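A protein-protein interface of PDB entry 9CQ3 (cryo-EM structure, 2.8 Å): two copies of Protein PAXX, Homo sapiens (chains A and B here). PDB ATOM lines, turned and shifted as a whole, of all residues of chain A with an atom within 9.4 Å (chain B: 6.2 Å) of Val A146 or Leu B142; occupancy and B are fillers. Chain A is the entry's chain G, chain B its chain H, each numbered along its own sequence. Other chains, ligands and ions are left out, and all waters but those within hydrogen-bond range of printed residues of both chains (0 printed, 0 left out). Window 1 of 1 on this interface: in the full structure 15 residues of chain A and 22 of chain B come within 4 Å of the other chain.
OE1 of Glu A150 lies within salt-bridge range of NH2 of Arg B145 (3.7 Å).
The backbone carbonyl oxygen of Leu A135 is in hydrogen-bond range of the side-chain hydroxyl of Thr A139.
Among the printed residues, pairs that only touch across the chains: Thr A24 with Ala B143, Pro A32 with Leu B140, Val A35 with Ala B143, Thr A139 with Thr B139, Val A146 with Leu B22, Val A146 with Leu B142, Val A146 with Arg B145, Val A146 with Val B146, Trp A147 with Leu B22, Leu A149 with Val B146, Leu A149 with Leu B149 and Leu A153 with Leu B149.
Ser A19 touches none of the printed residues of chain B.
Printed residues of chain B within 4 Å of Thr A24: Ala B143 (3.9 Å).
Ala A143 touches none of the printed residues of chain B.
Val A146 touches just these residues of chain B: Leu B22 (3.7 Å), Leu B142 (3.7 Å), Arg B145 (3.8 Å) and Val B146 (3.2 Å).
Of the printed residues of chain B, Leu A153 touches Leu B149 (3.3 Å).
Of the printed residues of chain A, Leu B22 touches Val A146 (3.7 Å) and Trp A147 (3.7 Å).
Leu B142 touches just one residue of chain A: Val A146.
Of chain A, only Thr A24 and Val A35 come within 4 Å of Ala B143.
Printed residues of chain A within 4 Å of Val B146: Val A146 and Leu A149.
The nearest residue of chain B that does not touch Val A146 is Leu B149 (5.6 Å).
The nearest residue of chain A that does not touch Leu B142 is Ala A143 (4.6 Å).
The nearest printed residue of chain B that does not touch Thr A24 is Trp B147 (4.6 Å).
Of the 13 printed residues of chain B, 8 touch a printed residue of chain A.
Of the 24 printed residues of chain A, 9 touch a printed residue of chain B.
Among the printed residues, 13 pairs touch across the chains.
Among the printed residues, Asp or Glu carboxylates within 4 Å of a Lys or Arg side-chain nitrogen of the other chain: Glu A150 with Arg B145.
Thr A139 touches its own counterpart, Thr B139.
Val A146 touches Leu B22, but with the chains exchanged Leu A22 does not touch Val B146 (4.5 Å).
Leu A149 touches Val B146, but with the chains exchanged Val A146 does not touch Leu B149 (5.6 Å).
Leu B149 touches its own counterpart, Leu A149.
Positions printed for both chains: 22, 138, 139, 140, 141, 142, 143, 144, 145, 146, 147 and 149.
Of the 13 pairs that touch across the chains among the printed residues, 3 have their exchanged pair printed and touching as well.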
ATOM      1  N   SER A  19     -25.063   7.519  -8.039  1.00  0.00           N
ATOM      2  CA  SER A  19     -23.970   8.483  -8.060  1.00  0.00           C
ATOM      3  C   SER A  19     -24.318   9.718  -7.234  1.00  0.00           C
ATOM      4  O   SER A  19     -24.605  10.779  -7.791  1.00  0.00           O
ATOM      5  CB  SER A  19     -23.643   8.891  -9.499  1.00  0.00           C
ATOM      6  OG  SER A  19     -23.013   7.831 -10.198  1.00  0.00           O
ATOM      7  N   LEU A  22     -20.873  14.661  -4.907  1.00  0.00           N
ATOM      8  CA  LEU A  22     -19.697  14.755  -4.055  1.00  0.00           C
ATOM      9  C   LEU A  22     -18.701  15.703  -4.704  1.00  0.00           C
ATOM     10  O   LEU A  22     -18.776  15.984  -5.903  1.00  0.00           O
ATOM     11  CB  LEU A  22     -19.062  13.379  -3.818  1.00  0.00           C
ATOM     12  CG  LEU A  22     -18.058  12.873  -4.858  1.00  0.00           C
ATOM     13  CD1 LEU A  22     -17.438  11.562  -4.399  1.00  0.00           C
ATOM     14  CD2 LEU A  22     -18.717  12.708  -6.219  1.00  0.00           C
ATOM     15  N   THR A  24     -14.322  17.236  -4.065  1.00  0.00           N
ATOM     16  CA  THR A  24     -13.054  17.189  -3.354  1.00  0.00           C
ATOM     17  C   THR A  24     -12.459  18.587  -3.257  1.00  0.00           C
ATOM     18  O   THR A  24     -12.576  19.391  -4.188  1.00  0.00           O
ATOM     19  CB  THR A  24     -12.063  16.254  -4.054  1.00  0.00           C
ATOM     20  OG1 THR A  24     -11.520  16.906  -5.209  1.00  0.00           O
ATOM     21  CG2 THR A  24     -12.750  14.964  -4.480  1.00  0.00           C
ATOM     22  N   PRO A  32      -5.592  16.108  -3.677  1.00  0.00           N
ATOM     23  CA  PRO A  32      -6.756  16.299  -2.805  1.00  0.00           C
ATOM     24  C   PRO A  32      -6.404  16.103  -1.339  1.00  0.00           C
ATOM     25  O   PRO A  32      -5.492  15.352  -0.986  1.00  0.00           O
ATOM     26  CB  PRO A  32      -7.741  15.228  -3.287  1.00  0.00           C
ATOM     27  CG  PRO A  32      -6.886  14.174  -3.890  1.00  0.00           C
ATOM     28  CD  PRO A  32      -5.708  14.886  -4.491  1.00  0.00           C
ATOM     29  N   VAL A  35     -12.714  15.254   1.054  1.00  0.00           N
ATOM     30  CA  VAL A  35     -13.784  14.827   0.155  1.00  0.00           C
ATOM     31  C   VAL A  35     -15.101  14.873   0.915  1.00  0.00           C
ATOM     32  O   VAL A  35     -15.195  14.359   2.034  1.00  0.00           O
ATOM     33  CB  VAL A  35     -13.532  13.416  -0.413  1.00  0.00           C
ATOM     34  CG1 VAL A  35     -12.185  13.360  -1.117  1.00  0.00           C
ATOM     35  CG2 VAL A  35     -13.606  12.370   0.689  1.00  0.00           C
ATOM     36  N   LEU A 135     -15.944   4.394   6.779  1.00  0.00           N
ATOM     37  CA  LEU A 135     -14.830   4.610   5.861  1.00  0.00           C
ATOM     38  C   LEU A 135     -14.660   3.430   4.912  1.00  0.00           C
ATOM     39  O   LEU A 135     -14.405   3.617   3.717  1.00  0.00           O
ATOM     40  CB  LEU A 135     -13.543   4.856   6.648  1.00  0.00           C
ATOM     41  CG  LEU A 135     -13.475   6.179   7.412  1.00  0.00           C
ATOM     42  CD1 LEU A 135     -12.344   6.152   8.429  1.00  0.00           C
ATOM     43  CD2 LEU A 135     -13.306   7.349   6.453  1.00  0.00           C
ATOM     44  N   ARG A 136     -14.788   2.205   5.427  1.00  0.00           N
ATOM     45  CA  ARG A 136     -14.669   1.031   4.567  1.00  0.00           C
ATOM     46  C   ARG A 136     -15.767   1.013   3.509  1.00  0.00           C
ATOM     47  O   ARG A 136     -15.505   0.739   2.329  1.00  0.00           O
ATOM     48  CB  ARG A 136     -14.718  -0.245   5.409  1.00  0.00           C
ATOM     49  CG  ARG A 136     -13.630  -0.337   6.472  1.00  0.00           C
ATOM     50  CD  ARG A 136     -14.025  -1.283   7.598  1.00  0.00           C
ATOM     51  NE  ARG A 136     -13.244  -1.053   8.808  1.00  0.00           N
ATOM     52  CZ  ARG A 136     -13.575  -1.503  10.012  1.00  0.00           C
ATOM     53  NH1 ARG A 136     -14.674  -2.212  10.208  1.00  0.00           N
ATOM     54  NH2 ARG A 136     -12.781  -1.233  11.044  1.00  0.00           N
ATOM     55  N   LEU A 138     -17.388   3.594   2.354  1.00  0.00           N
ATOM     56  CA  LEU A 138     -17.110   4.676   1.417  1.00  0.00           C
ATOM     57  C   LEU A 138     -16.040   4.268   0.413  1.00  0.00           C
ATOM     58  O   LEU A 138     -16.155   4.565  -0.779  1.00  0.00           O
ATOM     59  CB  LEU A 138     -16.682   5.930   2.182  1.00  0.00           C
ATOM     60  CG  LEU A 138     -16.027   7.048   1.368  1.00  0.00           C
ATOM     61  CD1 LEU A 138     -16.967   7.541   0.278  1.00  0.00           C
ATOM     62  CD2 LEU A 138     -15.610   8.192   2.278  1.00  0.00           C
ATOM     63  N   THR A 139     -14.987   3.595   0.879  1.00  0.00           N
ATOM     64  CA  THR A 139     -13.931   3.155  -0.029  1.00  0.00           C
ATOM     65  C   THR A 139     -14.467   2.155  -1.047  1.00  0.00           C
ATOM     66  O   THR A 139     -14.171   2.247  -2.245  1.00  0.00           O
ATOM     67  CB  THR A 139     -12.775   2.546   0.767  1.00  0.00           C
ATOM     68  OG1 THR A 139     -12.369   3.454   1.799  1.00  0.00           O
ATOM     69  CG2 THR A 139     -11.591   2.256  -0.145  1.00  0.00           C
ATOM     70  N   LEU A 140     -15.262   1.186  -0.583  1.00  0.00           N
ATOM     71  CA  LEU A 140     -15.829   0.206  -1.507  1.00  0.00           C
ATOM     72  C   LEU A 140     -16.743   0.879  -2.524  1.00  0.00           C
ATOM     73  O   LEU A 140     -16.688   0.573  -3.725  1.00  0.00           O
ATOM     74  CB  LEU A 140     -16.590  -0.868  -0.730  1.00  0.00           C
ATOM     75  CG  LEU A 140     -15.753  -1.750   0.199  1.00  0.00           C
ATOM     76  CD1 LEU A 140     -16.649  -2.689   0.992  1.00  0.00           C
ATOM     77  CD2 LEU A 140     -14.713  -2.537  -0.583  1.00  0.00           C
ATOM     78  N   GLY A 141     -17.586   1.804  -2.065  1.00  0.00           N
ATOM     79  CA  GLY A 141     -18.451   2.521  -2.984  1.00  0.00           C
ATOM     80  C   GLY A 141     -17.669   3.332  -3.998  1.00  0.00           C
ATOM     81  O   GLY A 141     -18.014   3.360  -5.179  1.00  0.00           O
ATOM     82  N   LEU A 142     -16.608   4.005  -3.549  1.00  0.00           N
ATOM     83  CA  LEU A 142     -15.786   4.788  -4.464  1.00  0.00           C
ATOM     84  C   LEU A 142     -15.141   3.897  -5.513  1.00  0.00           C
ATOM     85  O   LEU A 142     -15.080   4.259  -6.692  1.00  0.00           O
ATOM     86  CB  LEU A 142     -14.717   5.556  -3.686  1.00  0.00           C
ATOM     87  CG  LEU A 142     -15.220   6.705  -2.810  1.00  0.00           C
ATOM     88  CD1 LEU A 142     -14.248   6.968  -1.670  1.00  0.00           C
ATOM     89  CD2 LEU A 142     -15.431   7.961  -3.639  1.00  0.00           C
ATOM     90  N   ALA A 143     -14.648   2.726  -5.104  1.00  0.00           N
ATOM     91  CA  ALA A 143     -14.081   1.794  -6.074  1.00  0.00           C
ATOM     92  C   ALA A 143     -15.133   1.358  -7.088  1.00  0.00           C
ATOM     93  O   ALA A 143     -14.859   1.295  -8.295  1.00  0.00           O
ATOM     94  CB  ALA A 143     -13.492   0.582  -5.355  1.00  0.00           C
ATOM     95  N   LYS A 144     -16.345   1.054  -6.616  1.00  0.00           N
ATOM     96  CA  LYS A 144     -17.405   0.640  -7.533  1.00  0.00           C
ATOM     97  C   LYS A 144     -17.746   1.750  -8.520  1.00  0.00           C
ATOM     98  O   LYS A 144     -17.905   1.496  -9.722  1.00  0.00           O
ATOM     99  CB  LYS A 144     -18.647   0.226  -6.745  1.00  0.00           C
ATOM    100  CG  LYS A 144     -19.667  -0.547  -7.568  1.00  0.00           C
ATOM    101  CD  LYS A 144     -21.017  -0.608  -6.872  1.00  0.00           C
ATOM    102  CE  LYS A 144     -21.959  -1.574  -7.571  1.00  0.00           C
ATOM    103  NZ  LYS A 144     -22.233  -1.170  -8.978  1.00  0.00           N
ATOM    104  N   ARG A 145     -17.868   2.987  -8.033  1.00  0.00           N
ATOM    105  CA  ARG A 145     -18.177   4.102  -8.924  1.00  0.00           C
ATOM    106  C   ARG A 145     -17.052   4.330  -9.924  1.00  0.00           C
ATOM    107  O   ARG A 145     -17.306   4.631 -11.095  1.00  0.00           O
ATOM    108  CB  ARG A 145     -18.441   5.380  -8.123  1.00  0.00           C
ATOM    109  CG  ARG A 145     -19.456   5.227  -7.004  1.00  0.00           C
ATOM    110  CD  ARG A 145     -20.231   6.513  -6.759  1.00  0.00           C
ATOM    111  NE  ARG A 145     -20.970   6.468  -5.502  1.00  0.00           N
ATOM    112  CZ  ARG A 145     -20.412   6.449  -4.299  1.00  0.00           C
ATOM    113  NH1 ARG A 145     -19.098   6.499  -4.144  1.00  0.00           N
ATOM    114  NH2 ARG A 145     -21.190   6.381  -3.223  1.00  0.00           N
ATOM    115  N   VAL A 146     -15.800   4.201  -9.479  1.00  0.00           N
ATOM    116  CA  VAL A 146     -14.670   4.362 -10.388  1.00  0.00           C
ATOM    117  C   VAL A 146     -14.746   3.327 -11.500  1.00  0.00           C
ATOM    118  O   VAL A 146     -14.593   3.648 -12.685  1.00  0.00           O
ATOM    119  CB  VAL A 146     -13.342   4.263  -9.617  1.00  0.00           C
ATOM    120  CG1 VAL A 146     -12.192   3.925 -10.560  1.00  0.00           C
ATOM    121  CG2 VAL A 146     -13.061   5.558  -8.880  1.00  0.00           C
ATOM    122  N   TRP A 147     -14.991   2.067 -11.137  1.00  0.00           N
ATOM    123  CA  TRP A 147     -15.086   1.018 -12.146  1.00  0.00           C
ATOM    124  C   TRP A 147     -16.223   1.301 -13.120  1.00  0.00           C
ATOM    125  O   TRP A 147     -16.051   1.209 -14.344  1.00  0.00           O
ATOM    126  CB  TRP A 147     -15.277  -0.339 -11.467  1.00  0.00           C
ATOM    127  CG  TRP A 147     -15.762  -1.417 -12.390  1.00  0.00           C
ATOM    128  CD1 TRP A 147     -17.059  -1.758 -12.645  1.00  0.00           C
ATOM    129  CD2 TRP A 147     -14.953  -2.299 -13.179  1.00  0.00           C
ATOM    130  NE1 TRP A 147     -17.108  -2.795 -13.545  1.00  0.00           N
ATOM    131  CE2 TRP A 147     -15.829  -3.146 -13.888  1.00  0.00           C
ATOM    132  CE3 TRP A 147     -13.574  -2.455 -13.355  1.00  0.00           C
ATOM    133  CZ2 TRP A 147     -15.371  -4.132 -14.759  1.00  0.00           C
ATOM    134  CZ3 TRP A 147     -13.122  -3.434 -14.221  1.00  0.00           C
ATOM    135  CH2 TRP A 147     -14.018  -4.260 -14.911  1.00  0.00           C
ATOM    136  N   SER A 148     -17.396   1.660 -12.592  1.00  0.00           N
ATOM    137  CA  SER A 148     -18.557   1.880 -13.448  1.00  0.00           C
ATOM    138  C   SER A 148     -18.322   3.040 -14.409  1.00  0.00           C
ATOM    139  O   SER A 148     -18.603   2.936 -15.609  1.00  0.00           O
ATOM    140  CB  SER A 148     -19.796   2.136 -12.590  1.00  0.00           C
ATOM    141  OG  SER A 148     -20.054   3.524 -12.469  1.00  0.00           O
ATOM    142  N   LEU A 149     -17.800   4.158 -13.897  1.00  0.00           N
ATOM    143  CA  LEU A 149     -17.593   5.322 -14.751  1.00  0.00           C
ATOM    144  C   LEU A 149     -16.470   5.088 -15.752  1.00  0.00           C
ATOM    145  O   LEU A 149     -16.551   5.569 -16.886  1.00  0.00           O
ATOM    146  CB  LEU A 149     -17.307   6.559 -13.898  1.00  0.00           C
ATOM    147  CG  LEU A 149     -16.036   6.549 -13.047  1.00  0.00           C
ATOM    148  CD1 LEU A 149     -14.823   7.000 -13.847  1.00  0.00           C
ATOM    149  CD2 LEU A 149     -16.219   7.425 -11.818  1.00  0.00           C
ATOM    150  N   GLU A 150     -15.421   4.355 -15.366  1.00  0.00           N
ATOM    151  CA  GLU A 150     -14.376   4.020 -16.325  1.00  0.00           C
ATOM    152  C   GLU A 150     -14.930   3.161 -17.453  1.00  0.00           C
ATOM    153  O   GLU A 150     -14.631   3.398 -18.630  1.00  0.00           O
ATOM    154  CB  GLU A 150     -13.227   3.301 -15.617  1.00  0.00           C
ATOM    155  CG  GLU A 150     -12.030   3.014 -16.510  1.00  0.00           C
ATOM    156  CD  GLU A 150     -10.890   2.353 -15.760  1.00  0.00           C
ATOM    157  OE1 GLU A 150     -11.052   2.076 -14.554  1.00  0.00           O
ATOM    158  OE2 GLU A 150      -9.833   2.109 -16.379  1.00  0.00           O
ATOM    159  N   ARG A 151     -15.750   2.162 -17.115  1.00  0.00           N
ATOM    160  CA  ARG A 151     -16.354   1.333 -18.154  1.00  0.00           C
ATOM    161  C   ARG A 151     -17.259   2.161 -19.059  1.00  0.00           C
ATOM    162  O   ARG A 151     -17.235   2.006 -20.286  1.00  0.00           O
ATOM    163  CB  ARG A 151     -17.138   0.184 -17.519  1.00  0.00           C
ATOM    164  CG  ARG A 151     -17.094  -1.113 -18.316  1.00  0.00           C
ATOM    165  CD  ARG A 151     -17.340  -2.327 -17.432  1.00  0.00           C
ATOM    166  NE  ARG A 151     -18.755  -2.507 -17.131  1.00  0.00           N
ATOM    167  CZ  ARG A 151     -19.641  -3.027 -17.968  1.00  0.00           C
ATOM    168  NH1 ARG A 151     -19.295  -3.431 -19.181  1.00  0.00           N
ATOM    169  NH2 ARG A 151     -20.909  -3.146 -17.581  1.00  0.00           N
ATOM    170  N   ARG A 152     -18.061   3.052 -18.470  1.00  0.00           N
ATOM    171  CA  ARG A 152     -18.950   3.886 -19.273  1.00  0.00           C
ATOM    172  C   ARG A 152     -18.160   4.793 -20.208  1.00  0.00           C
ATOM    173  O   ARG A 152     -18.516   4.949 -21.382  1.00  0.00           O
ATOM    174  CB  ARG A 152     -19.853   4.715 -18.361  1.00  0.00           C
ATOM    175  CG  ARG A 152     -20.964   3.916 -17.698  1.00  0.00           C
ATOM    176  CD  ARG A 152     -21.786   4.782 -16.758  1.00  0.00           C
ATOM    177  NE  ARG A 152     -22.724   3.995 -15.967  1.00  0.00           N
ATOM    178  CZ  ARG A 152     -23.482   4.486 -14.996  1.00  0.00           C
ATOM    179  NH1 ARG A 152     -23.443   5.767 -14.665  1.00  0.00           N
ATOM    180  NH2 ARG A 152     -24.304   3.670 -14.340  1.00  0.00           N
ATOM    181  N   LEU A 153     -17.085   5.405 -19.705  1.00  0.00           N
ATOM    182  CA  LEU A 153     -16.269   6.276 -20.543  1.00  0.00           C
ATOM    183  C   LEU A 153     -15.607   5.490 -21.666  1.00  0.00           C
ATOM    184  O   LEU A 153     -15.552   5.955 -22.809  1.00  0.00           O
ATOM    185  CB  LEU A 153     -15.216   6.987 -19.691  1.00  0.00           C
ATOM    186  CG  LEU A 153     -14.297   7.963 -20.432  1.00  0.00           C
ATOM    187  CD1 LEU A 153     -15.097   9.096 -21.056  1.00  0.00           C
ATOM    188  CD2 LEU A 153     -13.234   8.511 -19.493  1.00  0.00           C
ATOM    189  N   ALA A 154     -15.102   4.293 -21.362  1.00  0.00           N
ATOM    190  CA  ALA A 154     -14.494   3.472 -22.403  1.00  0.00           C
ATOM    191  C   ALA A 154     -15.514   3.100 -23.470  1.00  0.00           C
ATOM    192  O   ALA A 154     -15.201   3.091 -24.666  1.00  0.00           O
ATOM    193  CB  ALA A 154     -13.877   2.216 -21.788  1.00  0.00           C
ATOM    194  N   LEU B  22      -7.437  -1.285 -12.680  1.00  0.00           N
ATOM    195  CA  LEU B  22      -8.022  -1.803 -11.451  1.00  0.00           C
ATOM    196  C   LEU B  22      -9.232  -2.651 -11.806  1.00  0.00           C
ATOM    197  O   LEU B  22      -9.784  -2.553 -12.905  1.00  0.00           O
ATOM    198  CB  LEU B  22      -8.415  -0.672 -10.494  1.00  0.00           C
ATOM    199  CG  LEU B  22      -9.544   0.246 -10.964  1.00  0.00           C
ATOM    200  CD1 LEU B  22     -10.861  -0.136 -10.304  1.00  0.00           C
ATOM    201  CD2 LEU B  22      -9.202   1.698 -10.679  1.00  0.00           C
ATOM    202  N   ALA B 137      -3.958   6.947   0.584  1.00  0.00           N
ATOM    203  CA  ALA B 137      -3.548   7.378  -0.746  1.00  0.00           C
ATOM    204  C   ALA B 137      -4.477   6.822  -1.814  1.00  0.00           C
ATOM    205  O   ALA B 137      -4.815   7.522  -2.776  1.00  0.00           O
ATOM    206  CB  ALA B 137      -2.106   6.947  -1.014  1.00  0.00           C
ATOM    207  N   LEU B 138      -4.893   5.561  -1.674  1.00  0.00           N
ATOM    208  CA  LEU B 138      -5.798   4.973  -2.654  1.00  0.00           C
ATOM    209  C   LEU B 138      -7.128   5.710  -2.680  1.00  0.00           C
ATOM    210  O   LEU B 138      -7.674   5.979  -3.753  1.00  0.00           O
ATOM    211  CB  LEU B 138      -6.016   3.492  -2.346  1.00  0.00           C
ATOM    212  CG  LEU B 138      -6.971   2.743  -3.280  1.00  0.00           C
ATOM    213  CD1 LEU B 138      -6.238   2.258  -4.522  1.00  0.00           C
ATOM    214  CD2 LEU B 138      -7.636   1.589  -2.547  1.00  0.00           C
ATOM    215  N   THR B 139      -7.671   6.040  -1.506  1.00  0.00           N
ATOM    216  CA  THR B 139      -8.937   6.764  -1.458  1.00  0.00           C
ATOM    217  C   THR B 139      -8.798   8.151  -2.072  1.00  0.00           C
ATOM    218  O   THR B 139      -9.666   8.591  -2.837  1.00  0.00           O
ATOM    219  CB  THR B 139      -9.429   6.866  -0.014  1.00  0.00           C
ATOM    220  OG1 THR B 139      -8.313   7.068   0.863  1.00  0.00           O
ATOM    221  CG2 THR B 139     -10.163   5.595   0.390  1.00  0.00           C
ATOM    222  N   LEU B 140      -7.707   8.855  -1.753  1.00  0.00           N
ATOM    223  CA  LEU B 140      -7.502  10.179  -2.330  1.00  0.00           C
ATOM    224  C   LEU B 140      -7.375  10.103  -3.848  1.00  0.00           C
ATOM    225  O   LEU B 140      -7.972  10.909  -4.572  1.00  0.00           O
ATOM    226  CB  LEU B 140      -6.263  10.829  -1.715  1.00  0.00           C
ATOM    227  CG  LEU B 140      -6.359  11.143  -0.221  1.00  0.00           C
ATOM    228  CD1 LEU B 140      -4.990  11.494   0.342  1.00  0.00           C
ATOM    229  CD2 LEU B 140      -7.350  12.269   0.033  1.00  0.00           C
ATOM    230  N   GLY B 141      -6.608   9.131  -4.346  1.00  0.00           N
ATOM    231  CA  GLY B 141      -6.461   8.980  -5.782  1.00  0.00           C
ATOM    232  C   GLY B 141      -7.760   8.599  -6.462  1.00  0.00           C
ATOM    233  O   GLY B 141      -8.054   9.069  -7.562  1.00  0.00           O
ATOM    234  N   LEU B 142      -8.552   7.736  -5.823  1.00  0.00           N
ATOM    235  CA  LEU B 142      -9.845   7.365  -6.386  1.00  0.00           C
ATOM    236  C   LEU B 142     -10.769   8.572  -6.467  1.00  0.00           C
ATOM    237  O   LEU B 142     -11.460   8.764  -7.472  1.00  0.00           O
ATOM    238  CB  LEU B 142     -10.483   6.257  -5.548  1.00  0.00           C
ATOM    239  CG  LEU B 142      -9.832   4.876  -5.659  1.00  0.00           C
ATOM    240  CD1 LEU B 142     -10.205   4.014  -4.463  1.00  0.00           C
ATOM    241  CD2 LEU B 142     -10.229   4.192  -6.957  1.00  0.00           C
ATOM    242  N   ALA B 143     -10.795   9.399  -5.419  1.00  0.00           N
ATOM    243  CA  ALA B 143     -11.620  10.602  -5.460  1.00  0.00           C
ATOM    244  C   ALA B 143     -11.155  11.549  -6.560  1.00  0.00           C
ATOM    245  O   ALA B 143     -11.975  12.109  -7.302  1.00  0.00           O
ATOM    246  CB  ALA B 143     -11.594  11.301  -4.102  1.00  0.00           C
ATOM    247  N   LYS B 144      -9.838  11.738  -6.684  1.00  0.00           N
ATOM    248  CA  LYS B 144      -9.317  12.614  -7.728  1.00  0.00           C
ATOM    249  C   LYS B 144      -9.670  12.087  -9.112  1.00  0.00           C
ATOM    250  O   LYS B 144     -10.057  12.857 -10.000  1.00  0.00           O
ATOM    251  CB  LYS B 144      -7.803  12.761  -7.580  1.00  0.00           C
ATOM    252  CG  LYS B 144      -7.128  13.451  -8.757  1.00  0.00           C
ATOM    253  CD  LYS B 144      -5.708  13.878  -8.413  1.00  0.00           C
ATOM    254  CE  LYS B 144      -5.197  14.950  -9.364  1.00  0.00           C
ATOM    255  NZ  LYS B 144      -4.137  15.788  -8.740  1.00  0.00           N
ATOM    256  N   ARG B 145      -9.535  10.776  -9.319  1.00  0.00           N
ATOM    257  CA  ARG B 145      -9.875  10.186 -10.608  1.00  0.00           C
ATOM    258  C   ARG B 145     -11.361  10.326 -10.899  1.00  0.00           C
ATOM    259  O   ARG B 145     -11.753  10.606 -12.036  1.00  0.00           O
ATOM    260  CB  ARG B 145      -9.459   8.715 -10.637  1.00  0.00           C
ATOM    261  CG  ARG B 145      -7.954   8.497 -10.659  1.00  0.00           C
ATOM    262  CD  ARG B 145      -7.542   7.555 -11.777  1.00  0.00           C
ATOM    263  NE  ARG B 145      -8.244   6.279 -11.708  1.00  0.00           N
ATOM    264  CZ  ARG B 145      -8.263   5.377 -12.681  1.00  0.00           C
ATOM    265  NH1 ARG B 145      -7.621   5.577 -13.822  1.00  0.00           N
ATOM    266  NH2 ARG B 145      -8.942   4.248 -12.506  1.00  0.00           N
ATOM    267  N   VAL B 146     -12.208  10.129  -9.886  1.00  0.00           N
ATOM    268  CA  VAL B 146     -13.643  10.307 -10.074  1.00  0.00           C
ATOM    269  C   VAL B 146     -13.934  11.728 -10.534  1.00  0.00           C
ATOM    270  O   VAL B 146     -14.661  11.950 -11.509  1.00  0.00           O
ATOM    271  CB  VAL B 146     -14.402   9.974  -8.777  1.00  0.00           C
ATOM    272  CG1 VAL B 146     -15.825  10.516  -8.833  1.00  0.00           C
ATOM    273  CG2 VAL B 146     -14.409   8.478  -8.531  1.00  0.00           C
ATOM    274  N   TRP B 147     -13.362  12.714  -9.840  1.00  0.00           N
ATOM    275  CA  TRP B 147     -13.609  14.106 -10.199  1.00  0.00           C
ATOM    276  C   TRP B 147     -13.127  14.401 -11.615  1.00  0.00           C
ATOM    277  O   TRP B 147     -13.845  15.011 -12.417  1.00  0.00           O
ATOM    278  CB  TRP B 147     -12.927  15.032  -9.192  1.00  0.00           C
ATOM    279  CG  TRP B 147     -13.239  16.481  -9.405  1.00  0.00           C
ATOM    280  CD1 TRP B 147     -14.273  17.186  -8.860  1.00  0.00           C
ATOM    281  CD2 TRP B 147     -12.512  17.405 -10.223  1.00  0.00           C
ATOM    282  NE1 TRP B 147     -14.234  18.491  -9.288  1.00  0.00           N
ATOM    283  CE2 TRP B 147     -13.162  18.652 -10.125  1.00  0.00           C
ATOM    284  CE3 TRP B 147     -11.373  17.299 -11.028  1.00  0.00           C
ATOM    285  CZ2 TRP B 147     -12.712  19.783 -10.802  1.00  0.00           C
ATOM    286  CZ3 TRP B 147     -10.929  18.425 -11.699  1.00  0.00           C
ATOM    287  CH2 TRP B 147     -11.597  19.650 -11.582  1.00  0.00           C
ATOM    288  N   LEU B 149     -12.540  12.342 -14.182  1.00  0.00           N
ATOM    289  CA  LEU B 149     -13.286  11.639 -15.219  1.00  0.00           C
ATOM    290  C   LEU B 149     -14.691  12.207 -15.368  1.00  0.00           C
ATOM    291  O   LEU B 149     -15.211  12.295 -16.485  1.00  0.00           O
ATOM    292  CB  LEU B 149     -13.326  10.144 -14.904  1.00  0.00           C
ATOM    293  CG  LEU B 149     -11.977   9.445 -15.104  1.00  0.00           C
ATOM    294  CD1 LEU B 149     -11.824   8.234 -14.195  1.00  0.00           C
ATOM    295  CD2 LEU B 149     -11.801   9.045 -16.561  1.00  0.00           C
